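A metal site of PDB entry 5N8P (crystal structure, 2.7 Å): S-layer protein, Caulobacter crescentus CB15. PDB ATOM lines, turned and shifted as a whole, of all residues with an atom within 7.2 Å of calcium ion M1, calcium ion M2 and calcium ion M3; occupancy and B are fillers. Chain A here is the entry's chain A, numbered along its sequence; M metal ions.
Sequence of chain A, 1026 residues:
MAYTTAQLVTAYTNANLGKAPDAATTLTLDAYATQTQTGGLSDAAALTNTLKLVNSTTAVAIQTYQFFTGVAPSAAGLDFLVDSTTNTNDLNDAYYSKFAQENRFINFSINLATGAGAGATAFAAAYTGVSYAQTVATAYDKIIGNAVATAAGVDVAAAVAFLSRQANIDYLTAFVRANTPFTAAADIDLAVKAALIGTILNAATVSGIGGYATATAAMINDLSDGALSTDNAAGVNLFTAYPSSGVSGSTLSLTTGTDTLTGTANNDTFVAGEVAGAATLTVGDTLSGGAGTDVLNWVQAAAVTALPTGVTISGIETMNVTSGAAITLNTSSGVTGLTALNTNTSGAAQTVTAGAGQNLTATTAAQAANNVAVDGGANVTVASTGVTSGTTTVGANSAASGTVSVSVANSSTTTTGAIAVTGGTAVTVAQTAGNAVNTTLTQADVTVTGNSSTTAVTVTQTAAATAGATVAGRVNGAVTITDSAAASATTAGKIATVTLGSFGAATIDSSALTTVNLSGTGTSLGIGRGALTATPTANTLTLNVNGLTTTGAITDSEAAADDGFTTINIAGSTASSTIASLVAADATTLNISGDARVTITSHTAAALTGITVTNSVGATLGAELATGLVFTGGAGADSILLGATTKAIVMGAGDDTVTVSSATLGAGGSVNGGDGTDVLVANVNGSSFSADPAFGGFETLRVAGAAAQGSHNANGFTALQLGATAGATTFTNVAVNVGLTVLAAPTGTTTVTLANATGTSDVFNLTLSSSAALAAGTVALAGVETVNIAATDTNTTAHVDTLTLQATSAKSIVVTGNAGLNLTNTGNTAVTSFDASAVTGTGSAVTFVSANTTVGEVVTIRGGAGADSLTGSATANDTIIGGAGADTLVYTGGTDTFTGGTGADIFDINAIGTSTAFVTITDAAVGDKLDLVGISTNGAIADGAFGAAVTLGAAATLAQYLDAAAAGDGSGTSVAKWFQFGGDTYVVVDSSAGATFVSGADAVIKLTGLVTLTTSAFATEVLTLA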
ATOM      1  N   SER A 844       2.883   6.275   8.492  1.00  0.00           N
ATOM      2  CA  SER A 844       3.496   4.945   8.448  1.00  0.00           C
ATOM      3  C   SER A 844       4.458   4.689   9.657  1.00  0.00           C
ATOM      4  O   SER A 844       5.710   4.709   9.574  1.00  0.00           O
ATOM      5  CB  SER A 844       4.066   4.540   7.055  1.00  0.00           C
ATOM      6  OG  SER A 844       4.451   5.565   6.162  1.00  0.00           O
ATOM      7  N   VAL A 846       6.554   3.287  12.655  1.00  0.00           N
ATOM      8  CA  VAL A 846       7.421   2.141  12.891  1.00  0.00           C
ATOM      9  C   VAL A 846       7.690   1.961  14.375  1.00  0.00           C
ATOM     10  O   VAL A 846       8.075   2.902  15.048  1.00  0.00           O
ATOM     11  CB  VAL A 846       8.715   2.293  12.080  1.00  0.00           C
ATOM     12  CG1 VAL A 846       9.709   1.184  12.409  1.00  0.00           C
ATOM     13  CG2 VAL A 846       8.402   2.367  10.576  1.00  0.00           C
ATOM     14  N   ARG A 862      17.112   3.771  13.152  1.00  0.00           N
ATOM     15  CA  ARG A 862      16.578   4.820  12.265  1.00  0.00           C
ATOM     16  C   ARG A 862      15.061   4.740  12.025  1.00  0.00           C
ATOM     17  O   ARG A 862      14.593   3.754  11.483  1.00  0.00           O
ATOM     18  CB  ARG A 862      17.310   4.775  10.917  1.00  0.00           C
ATOM     19  CG  ARG A 862      18.057   6.027  10.550  1.00  0.00           C
ATOM     20  CD  ARG A 862      19.477   5.911  11.025  1.00  0.00           C
ATOM     21  NE  ARG A 862      20.378   5.105  10.175  1.00  0.00           N
ATOM     22  CZ  ARG A 862      21.287   5.624   9.336  1.00  0.00           C
ATOM     23  NH1 ARG A 862      22.018   4.827   8.584  1.00  0.00           N
ATOM     24  NH2 ARG A 862      21.493   6.941   9.264  1.00  0.00           N
ATOM     25  N   GLY A 863      14.322   5.772  12.382  1.00  0.00           N
ATOM     26  CA  GLY A 863      12.895   5.908  12.071  1.00  0.00           C
ATOM     27  C   GLY A 863      12.616   6.473  10.678  1.00  0.00           C
ATOM     28  O   GLY A 863      13.532   6.883   9.943  1.00  0.00           O
ATOM     29  N   GLY A 864      11.333   6.485  10.309  1.00  0.00           N
ATOM     30  CA  GLY A 864      10.878   6.946   8.996  1.00  0.00           C
ATOM     31  C   GLY A 864      10.001   8.169   9.081  1.00  0.00           C
ATOM     32  O   GLY A 864      10.106   8.933  10.038  1.00  0.00           O
ATOM     33  N   ALA A 865       9.157   8.397   8.088  1.00  0.00           N
ATOM     34  CA  ALA A 865       8.284   9.577   8.090  1.00  0.00           C
ATOM     35  C   ALA A 865       7.175   9.512   9.174  1.00  0.00           C
ATOM     36  O   ALA A 865       6.604  10.532   9.546  1.00  0.00           O
ATOM     37  CB  ALA A 865       7.721   9.839   6.719  1.00  0.00           C
ATOM     38  N   GLY A 866       6.903   8.329   9.710  1.00  0.00           N
ATOM     39  CA  GLY A 866       5.799   8.116  10.655  1.00  0.00           C
ATOM     40  C   GLY A 866       6.119   8.523  12.072  1.00  0.00           C
ATOM     41  O   GLY A 866       7.241   8.831  12.394  1.00  0.00           O
ATOM     42  N   ALA A 867       5.083   8.536  12.894  1.00  0.00           N
ATOM     43  CA  ALA A 867       5.230   8.826  14.331  1.00  0.00           C
ATOM     44  C   ALA A 867       5.806   7.559  14.980  1.00  0.00           C
ATOM     45  O   ALA A 867       5.033   6.705  15.457  1.00  0.00           O
ATOM     46  CB  ALA A 867       3.872   9.213  14.949  1.00  0.00           C
ATOM     47  N   ASP A 868       7.135   7.437  14.987  1.00  0.00           N
ATOM     48  CA  ASP A 868       7.801   6.151  15.327  1.00  0.00           C
ATOM     49  C   ASP A 868       8.096   5.968  16.832  1.00  0.00           C
ATOM     50  O   ASP A 868       8.150   6.932  17.594  1.00  0.00           O
ATOM     51  CB  ASP A 868       9.089   5.943  14.519  1.00  0.00           C
ATOM     52  CG  ASP A 868       8.912   6.225  13.019  1.00  0.00           C
ATOM     53  OD1 ASP A 868       8.076   5.601  12.295  1.00  0.00           O
ATOM     54  OD2 ASP A 868       9.639   7.103  12.540  1.00  0.00           O
ATOM     55  N   SER A 869       8.301   4.712  17.249  1.00  0.00           N
ATOM     56  CA  SER A 869       8.559   4.403  18.650  1.00  0.00           C
ATOM     57  C   SER A 869       9.760   3.467  18.820  1.00  0.00           C
ATOM     58  O   SER A 869       9.642   2.232  18.834  1.00  0.00           O
ATOM     59  CB  SER A 869       7.306   3.864  19.338  1.00  0.00           C
ATOM     60  OG  SER A 869       7.610   3.485  20.667  1.00  0.00           O
ATOM     61  N   LEU A 870      10.916   4.098  18.991  1.00  0.00           N
ATOM     62  CA  LEU A 870      12.200   3.452  18.929  1.00  0.00           C
ATOM     63  C   LEU A 870      12.839   3.345  20.317  1.00  0.00           C
ATOM     64  O   LEU A 870      13.099   4.365  20.961  1.00  0.00           O
ATOM     65  CB  LEU A 870      13.082   4.242  17.951  1.00  0.00           C
ATOM     66  CG  LEU A 870      12.430   4.712  16.633  1.00  0.00           C
ATOM     67  CD1 LEU A 870      13.308   5.663  15.869  1.00  0.00           C
ATOM     68  CD2 LEU A 870      12.034   3.547  15.754  1.00  0.00           C
ATOM     69  N   ILE A 881      17.538   7.768  15.685  1.00  0.00           N
ATOM     70  CA  ILE A 881      17.163   8.899  14.828  1.00  0.00           C
ATOM     71  C   ILE A 881      15.739   8.697  14.301  1.00  0.00           C
ATOM     72  O   ILE A 881      15.543   7.832  13.463  1.00  0.00           O
ATOM     73  CB  ILE A 881      18.150   9.054  13.639  1.00  0.00           C
ATOM     74  CG1 ILE A 881      19.513   9.519  14.134  1.00  0.00           C
ATOM     75  CG2 ILE A 881      17.669   9.998  12.545  1.00  0.00           C
ATOM     76  CD1 ILE A 881      20.686   8.899  13.446  1.00  0.00           C
ATOM     77  N   GLY A 882      14.752   9.452  14.787  1.00  0.00           N
ATOM     78  CA  GLY A 882      13.396   9.497  14.144  1.00  0.00           C
ATOM     79  C   GLY A 882      13.449  10.295  12.841  1.00  0.00           C
ATOM     80  O   GLY A 882      14.402  11.018  12.585  1.00  0.00           O
ATOM     81  N   GLY A 883      12.449  10.198  12.002  1.00  0.00           N
ATOM     82  CA  GLY A 883      12.490  11.006  10.754  1.00  0.00           C
ATOM     83  C   GLY A 883      11.723  12.298  10.877  1.00  0.00           C
ATOM     84  O   GLY A 883      12.034  13.141  11.701  1.00  0.00           O
ATOM     85  N   ALA A 884      10.711  12.441  10.020  1.00  0.00           N
ATOM     86  CA  ALA A 884       9.619  13.395  10.215  1.00  0.00           C
ATOM     87  C   ALA A 884       8.727  12.879  11.360  1.00  0.00           C
ATOM     88  O   ALA A 884       9.000  11.795  11.900  1.00  0.00           O
ATOM     89  CB  ALA A 884       8.841  13.603   8.913  1.00  0.00           C
ATOM     90  N   GLY A 885       7.698  13.656  11.777  1.00  0.00           N
ATOM     91  CA  GLY A 885       6.652  13.142  12.681  1.00  0.00           C
ATOM     92  C   GLY A 885       6.995  12.921  14.150  1.00  0.00           C
ATOM     93  O   GLY A 885       8.155  12.980  14.555  1.00  0.00           O
ATOM     94  N   ALA A 886       5.959  12.670  14.941  1.00  0.00           N
ATOM     95  CA  ALA A 886       6.026  12.673  16.417  1.00  0.00           C
ATOM     96  C   ALA A 886       6.723  11.416  16.998  1.00  0.00           C
ATOM     97  O   ALA A 886       6.062  10.473  17.450  1.00  0.00           O
ATOM     98  CB  ALA A 886       4.613  12.869  17.027  1.00  0.00           C
ATOM     99  N   ASP A 887       8.054  11.420  16.980  1.00  0.00           N
ATOM    100  CA  ASP A 887       8.821  10.242  17.367  1.00  0.00           C
ATOM    101  C   ASP A 887       8.999  10.151  18.862  1.00  0.00           C
ATOM    102  O   ASP A 887       9.117  11.178  19.535  1.00  0.00           O
ATOM    103  CB  ASP A 887      10.172  10.228  16.675  1.00  0.00           C
ATOM    104  CG  ASP A 887      10.060  10.230  15.168  1.00  0.00           C
ATOM    105  OD1 ASP A 887       9.445   9.275  14.627  1.00  0.00           O
ATOM    106  OD2 ASP A 887      10.585  11.156  14.523  1.00  0.00           O
ATOM    107  N   THR A 888       8.960   8.923  19.384  1.00  0.00           N
ATOM    108  CA  THR A 888       9.312   8.637  20.778  1.00  0.00           C
ATOM    109  C   THR A 888      10.632   7.841  20.796  1.00  0.00           C
ATOM    110  O   THR A 888      10.696   6.741  20.238  1.00  0.00           O
ATOM    111  CB  THR A 888       8.148   7.940  21.545  1.00  0.00           C
ATOM    112  OG1 THR A 888       6.995   8.790  21.539  1.00  0.00           O
ATOM    113  CG2 THR A 888       8.522   7.641  23.036  1.00  0.00           C
ATOM    114  N   LEU A 889      11.662   8.427  21.401  1.00  0.00           N
ATOM    115  CA  LEU A 889      12.980   7.820  21.505  1.00  0.00           C
ATOM    116  C   LEU A 889      13.211   7.470  22.960  1.00  0.00           C
ATOM    117  O   LEU A 889      13.150   8.334  23.819  1.00  0.00           O
ATOM    118  CB  LEU A 889      14.024   8.815  21.013  1.00  0.00           C
ATOM    119  CG  LEU A 889      14.223   8.996  19.501  1.00  0.00           C
ATOM    120  CD1 LEU A 889      13.014   9.543  18.771  1.00  0.00           C
ATOM    121  CD2 LEU A 889      15.414   9.898  19.239  1.00  0.00           C
ATOM    122  N   THR A 899      18.386  11.899  18.096  1.00  0.00           N
ATOM    123  CA  THR A 899      18.031  12.920  17.132  1.00  0.00           C
ATOM    124  C   THR A 899      16.602  12.612  16.728  1.00  0.00           C
ATOM    125  O   THR A 899      16.368  11.660  15.993  1.00  0.00           O
ATOM    126  CB  THR A 899      18.977  12.871  15.902  1.00  0.00           C
ATOM    127  OG1 THR A 899      20.344  12.971  16.322  1.00  0.00           O
ATOM    128  CG2 THR A 899      18.653  13.958  14.881  1.00  0.00           C
ATOM    129  N   GLY A 900      15.641  13.350  17.265  1.00  0.00           N
ATOM    130  CA  GLY A 900      14.276  13.279  16.717  1.00  0.00           C
ATOM    131  C   GLY A 900      14.369  14.332  15.656  1.00  0.00           C
ATOM    132  O   GLY A 900      14.845  15.416  15.971  1.00  0.00           O
ATOM    133  N   GLY A 901      13.987  14.063  14.418  1.00  0.00           N
ATOM    134  CA  GLY A 901      14.150  15.051  13.343  1.00  0.00           C
ATOM    135  C   GLY A 901      13.141  16.186  13.464  1.00  0.00           C
ATOM    136  O   GLY A 901      12.972  16.808  14.526  1.00  0.00           O
ATOM    137  N   THR A 902      12.458  16.447  12.360  1.00  0.00           N
ATOM    138  CA  THR A 902      11.352  17.397  12.352  1.00  0.00           C
ATOM    139  C   THR A 902      10.191  16.845  13.226  1.00  0.00           C
ATOM    140  O   THR A 902      10.124  15.626  13.475  1.00  0.00           O
ATOM    141  CB  THR A 902      10.913  17.705  10.904  1.00  0.00           C
ATOM    142  OG1 THR A 902      10.153  16.603  10.375  1.00  0.00           O
ATOM    143  CG2 THR A 902      12.128  17.944   9.983  1.00  0.00           C
ATOM    144  N   GLY A 903       9.329  17.747  13.714  1.00  0.00           N
ATOM    145  CA  GLY A 903       8.144  17.352  14.481  1.00  0.00           C
ATOM    146  C   GLY A 903       8.297  17.336  15.990  1.00  0.00           C
ATOM    147  O   GLY A 903       9.404  17.412  16.515  1.00  0.00           O
ATOM    148  N   ALA A 904       7.155  17.248  16.684  1.00  0.00           N
ATOM    149  CA  ALA A 904       7.083  17.254  18.145  1.00  0.00           C
ATOM    150  C   ALA A 904       7.556  15.918  18.702  1.00  0.00           C
ATOM    151  O   ALA A 904       6.741  15.032  19.000  1.00  0.00           O
ATOM    152  CB  ALA A 904       5.638  17.555  18.593  1.00  0.00           C
ATOM    153  N   ASP A 905       8.875  15.752  18.840  1.00  0.00           N
ATOM    154  CA  ASP A 905       9.428  14.485  19.318  1.00  0.00           C
ATOM    155  C   ASP A 905       9.391  14.390  20.829  1.00  0.00           C
ATOM    156  O   ASP A 905       9.427  15.413  21.499  1.00  0.00           O
ATOM    157  CB  ASP A 905      10.850  14.294  18.794  1.00  0.00           C
ATOM    158  CG  ASP A 905      10.917  14.368  17.288  1.00  0.00           C
ATOM    159  OD1 ASP A 905      10.397  13.452  16.620  1.00  0.00           O
ATOM    160  OD2 ASP A 905      11.487  15.342  16.783  1.00  0.00           O
ATOM    161  N   ILE A 906       9.257  13.185  21.351  1.00  0.00           N
ATOM    162  CA  ILE A 906       9.294  13.009  22.811  1.00  0.00           C
ATOM    163  C   ILE A 906      10.517  12.134  23.196  1.00  0.00           C
ATOM    164  O   ILE A 906      10.688  11.033  22.685  1.00  0.00           O
ATOM    165  CB  ILE A 906       7.873  12.696  23.465  1.00  0.00           C
ATOM    166  CG1 ILE A 906       7.913  11.539  24.517  1.00  0.00           C
ATOM    167  CG2 ILE A 906       6.736  12.571  22.417  1.00  0.00           C
ATOM    168  CD1 ILE A 906       6.583  11.228  25.224  1.00  0.00           C
ATOM    169  N   PHE A 907      11.420  12.689  24.019  1.00  0.00           N
ATOM    170  CA  PHE A 907      12.609  11.956  24.470  1.00  0.00           C
ATOM    171  C   PHE A 907      12.300  11.354  25.826  1.00  0.00           C
ATOM    172  O   PHE A 907      12.387  12.046  26.843  1.00  0.00           O
ATOM    173  CB  PHE A 907      13.824  12.864  24.520  1.00  0.00           C
ATOM    174  CG  PHE A 907      14.104  13.524  23.215  1.00  0.00           C
ATOM    175  CD1 PHE A 907      14.691  12.818  22.165  1.00  0.00           C
ATOM    176  CD2 PHE A 907      13.753  14.853  22.999  1.00  0.00           C
ATOM    177  CE1 PHE A 907      14.957  13.416  20.948  1.00  0.00           C
ATOM    178  CE2 PHE A 907      14.006  15.469  21.771  1.00  0.00           C
ATOM    179  CZ  PHE A 907      14.606  14.746  20.732  1.00  0.00           C
ATOM    180  N   ASP A 923      19.441  17.617  18.806  1.00  0.00           N
ATOM    181  CA  ASP A 923      18.684  18.681  18.122  1.00  0.00           C
ATOM    182  C   ASP A 923      17.431  19.186  18.816  1.00  0.00           C
ATOM    183  O   ASP A 923      16.504  19.680  18.139  1.00  0.00           O
ATOM    184  CB  ASP A 923      18.348  18.237  16.674  1.00  0.00           C
ATOM    185  CG  ASP A 923      17.362  17.050  16.610  1.00  0.00           C
ATOM    186  OD1 ASP A 923      16.927  16.449  17.658  1.00  0.00           O
ATOM    187  OD2 ASP A 923      17.035  16.728  15.460  1.00  0.00           O
ATOM    188  N   ALA A 924      17.396  19.049  20.142  1.00  0.00           N
ATOM    189  CA  ALA A 924      16.298  19.588  20.964  1.00  0.00           C
ATOM    190  C   ALA A 924      15.898  21.003  20.501  1.00  0.00           C
ATOM    191  O   ALA A 924      16.732  21.896  20.397  1.00  0.00           O
ATOM    192  CB  ALA A 924      16.679  19.584  22.431  1.00  0.00           C
ATOM    193  N   ALA A 925      14.634  21.142  20.161  1.00  0.00           N
ATOM    194  CA  ALA A 925      14.093  22.390  19.613  1.00  0.00           C
ATOM    195  C   ALA A 925      12.695  22.633  20.166  1.00  0.00           C
ATOM    196  O   ALA A 925      12.113  21.767  20.828  1.00  0.00           O
ATOM    197  CB  ALA A 925      14.079  22.363  18.084  1.00  0.00           C
ATOM    198  N   VAL A 926      12.191  23.839  19.918  1.00  0.00           N
ATOM    199  CA  VAL A 926      10.853  24.243  20.300  1.00  0.00           C
ATOM    200  C   VAL A 926       9.799  23.207  19.832  1.00  0.00           C
ATOM    201  O   VAL A 926       9.729  22.856  18.639  1.00  0.00           O
ATOM    202  CB  VAL A 926      10.575  25.696  19.813  1.00  0.00           C
ATOM    203  CG1 VAL A 926      10.714  25.840  18.283  1.00  0.00           C
ATOM    204  CG2 VAL A 926       9.229  26.213  20.320  1.00  0.00           C
ATOM    205  N   GLY A 927       9.027  22.693  20.791  1.00  0.00           N
ATOM    206  CA  GLY A 927       7.982  21.693  20.512  1.00  0.00           C
ATOM    207  C   GLY A 927       8.284  20.284  21.012  1.00  0.00           C
ATOM    208  O   GLY A 927       7.366  19.567  21.436  1.00  0.00           O
ATOM    209  N   ASP A 928       9.564  19.912  20.960  1.00  0.00           N
ATOM    210  CA  ASP A 928      10.036  18.641  21.515  1.00  0.00           C
ATOM    211  C   ASP A 928       9.822  18.565  23.022  1.00  0.00           C
ATOM    212  O   ASP A 928       9.826  19.605  23.694  1.00  0.00           O
ATOM    213  CB  ASP A 928      11.514  18.400  21.160  1.00  0.00           C
ATOM    214  CG  ASP A 928      11.768  18.263  19.645  1.00  0.00           C
ATOM    215  OD1 ASP A 928      12.782  18.789  19.144  1.00  0.00           O
ATOM    216  OD2 ASP A 928      10.973  17.625  18.923  1.00  0.00           O
HETATM  217 CA    CA M   1      11.839  17.643  16.590  1.00  0.00          CA
HETATM  218 CA    CA M   2      10.895  13.401  14.166  1.00  0.00          CA
HETATM  219 CA    CA M   3       9.681   9.417  12.407  1.00  0.00          CA
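Calcium ion M3 is bound by OD1 of Asp 887 (2.2 Å). OD2 of Asp 868 binds calcium ion M3, 2.3 Å away. Calcium ion M3 is bound by O of Gly 864 (2.5 Å). Calcium ion M3 is bound by O of Gly 866, at 2.5 Å. Calcium ion M3 is bound by the backbone carbonyl oxygen (O) of Ala 884 (2.5 Å). OD2 of Asp 887 binds calcium ion M3 (2.9 Å). Slightly farther from calcium ion M3 lies N of Gly 883 (2.9 Å).
The backbone NH of Ile 906 lies within hydrogen-bond range of the backbone carbonyl oxygen of Asp 887 (2.7 Å). N of Val 846 lies within hydrogen-bond range of OD1 of Asp 868 (2.8 Å). N of Thr 888 lies within hydrogen-bond range of O of Asp 868 (2.8 Å). The backbone carbonyl oxygen (O) of Gly 864 sits close to the backbone NH (N) of Gly 883 (3.3 Å). The side-chain carboxylate of Asp 928 lies within hydrogen-bond range of the backbone NH of Ala 925, at 3.2 Å. N of Gly 901 sits close to O of Gly 883 (3.5 Å). OD1 of Asp 923 lies within hydrogen-bond range of N of Gly 900 (3.4 Å). The backbone carbonyl oxygen of Thr 899 sits at hydrogen-bond distance from the backbone NH of Gly 882, at 3.0 Å.
Merely in contact with calcium ion M1: Gly 900 (3.8 Å). Of the 35 residues printed, 6 come within 4 Å of calcium ion M1. Along chain A the residues within 4 Å of calcium ion M1 span positions 900 to 928.
Merely in contact with calcium ion M2: Gly 900. Eight residues have an atom within 4 Å of calcium ion M2: Gly 883, Ala 884, Gly 885, Asp 887, Gly 900, Gly 901, Thr 902 and Asp 905. Along chain A the residues within 4 Å of calcium ion M2 span positions 883 to 905. The nearest printed residue that does not touch calcium ion M2 is Gly 882 (4.2 Å).
Merely in contact with calcium ion M3: Gly 882. Within 4 Å of calcium ion M3: Gly 864, Gly 866, Asp 868, Gly 882, Gly 883, Ala 884 and Asp 887.
Calcium ion M1 is bound by OD2 of Asp 905 (2.3 Å), O of Gly 903 (2.4 Å), OD2 of Asp 928 (2.5 Å) and O of Gly 901 (2.5 Å). Slightly farther from calcium ion M1 lies OD1 of Asp 928 (3.0 Å).
OD2 of Asp 887 binds calcium ion M2 (2.3 Å). Calcium ion M2 is bound by O of Thr 902. Calcium ion M2 is bound by the side-chain carboxylate (OD1) of Asp 905. Calcium ion M2 is bound by O of Gly 883. The backbone carbonyl oxygen (O) of Gly 885 binds calcium ion M2 (2.8 Å). Calcium ion M2 has five donor atoms within binding distance.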
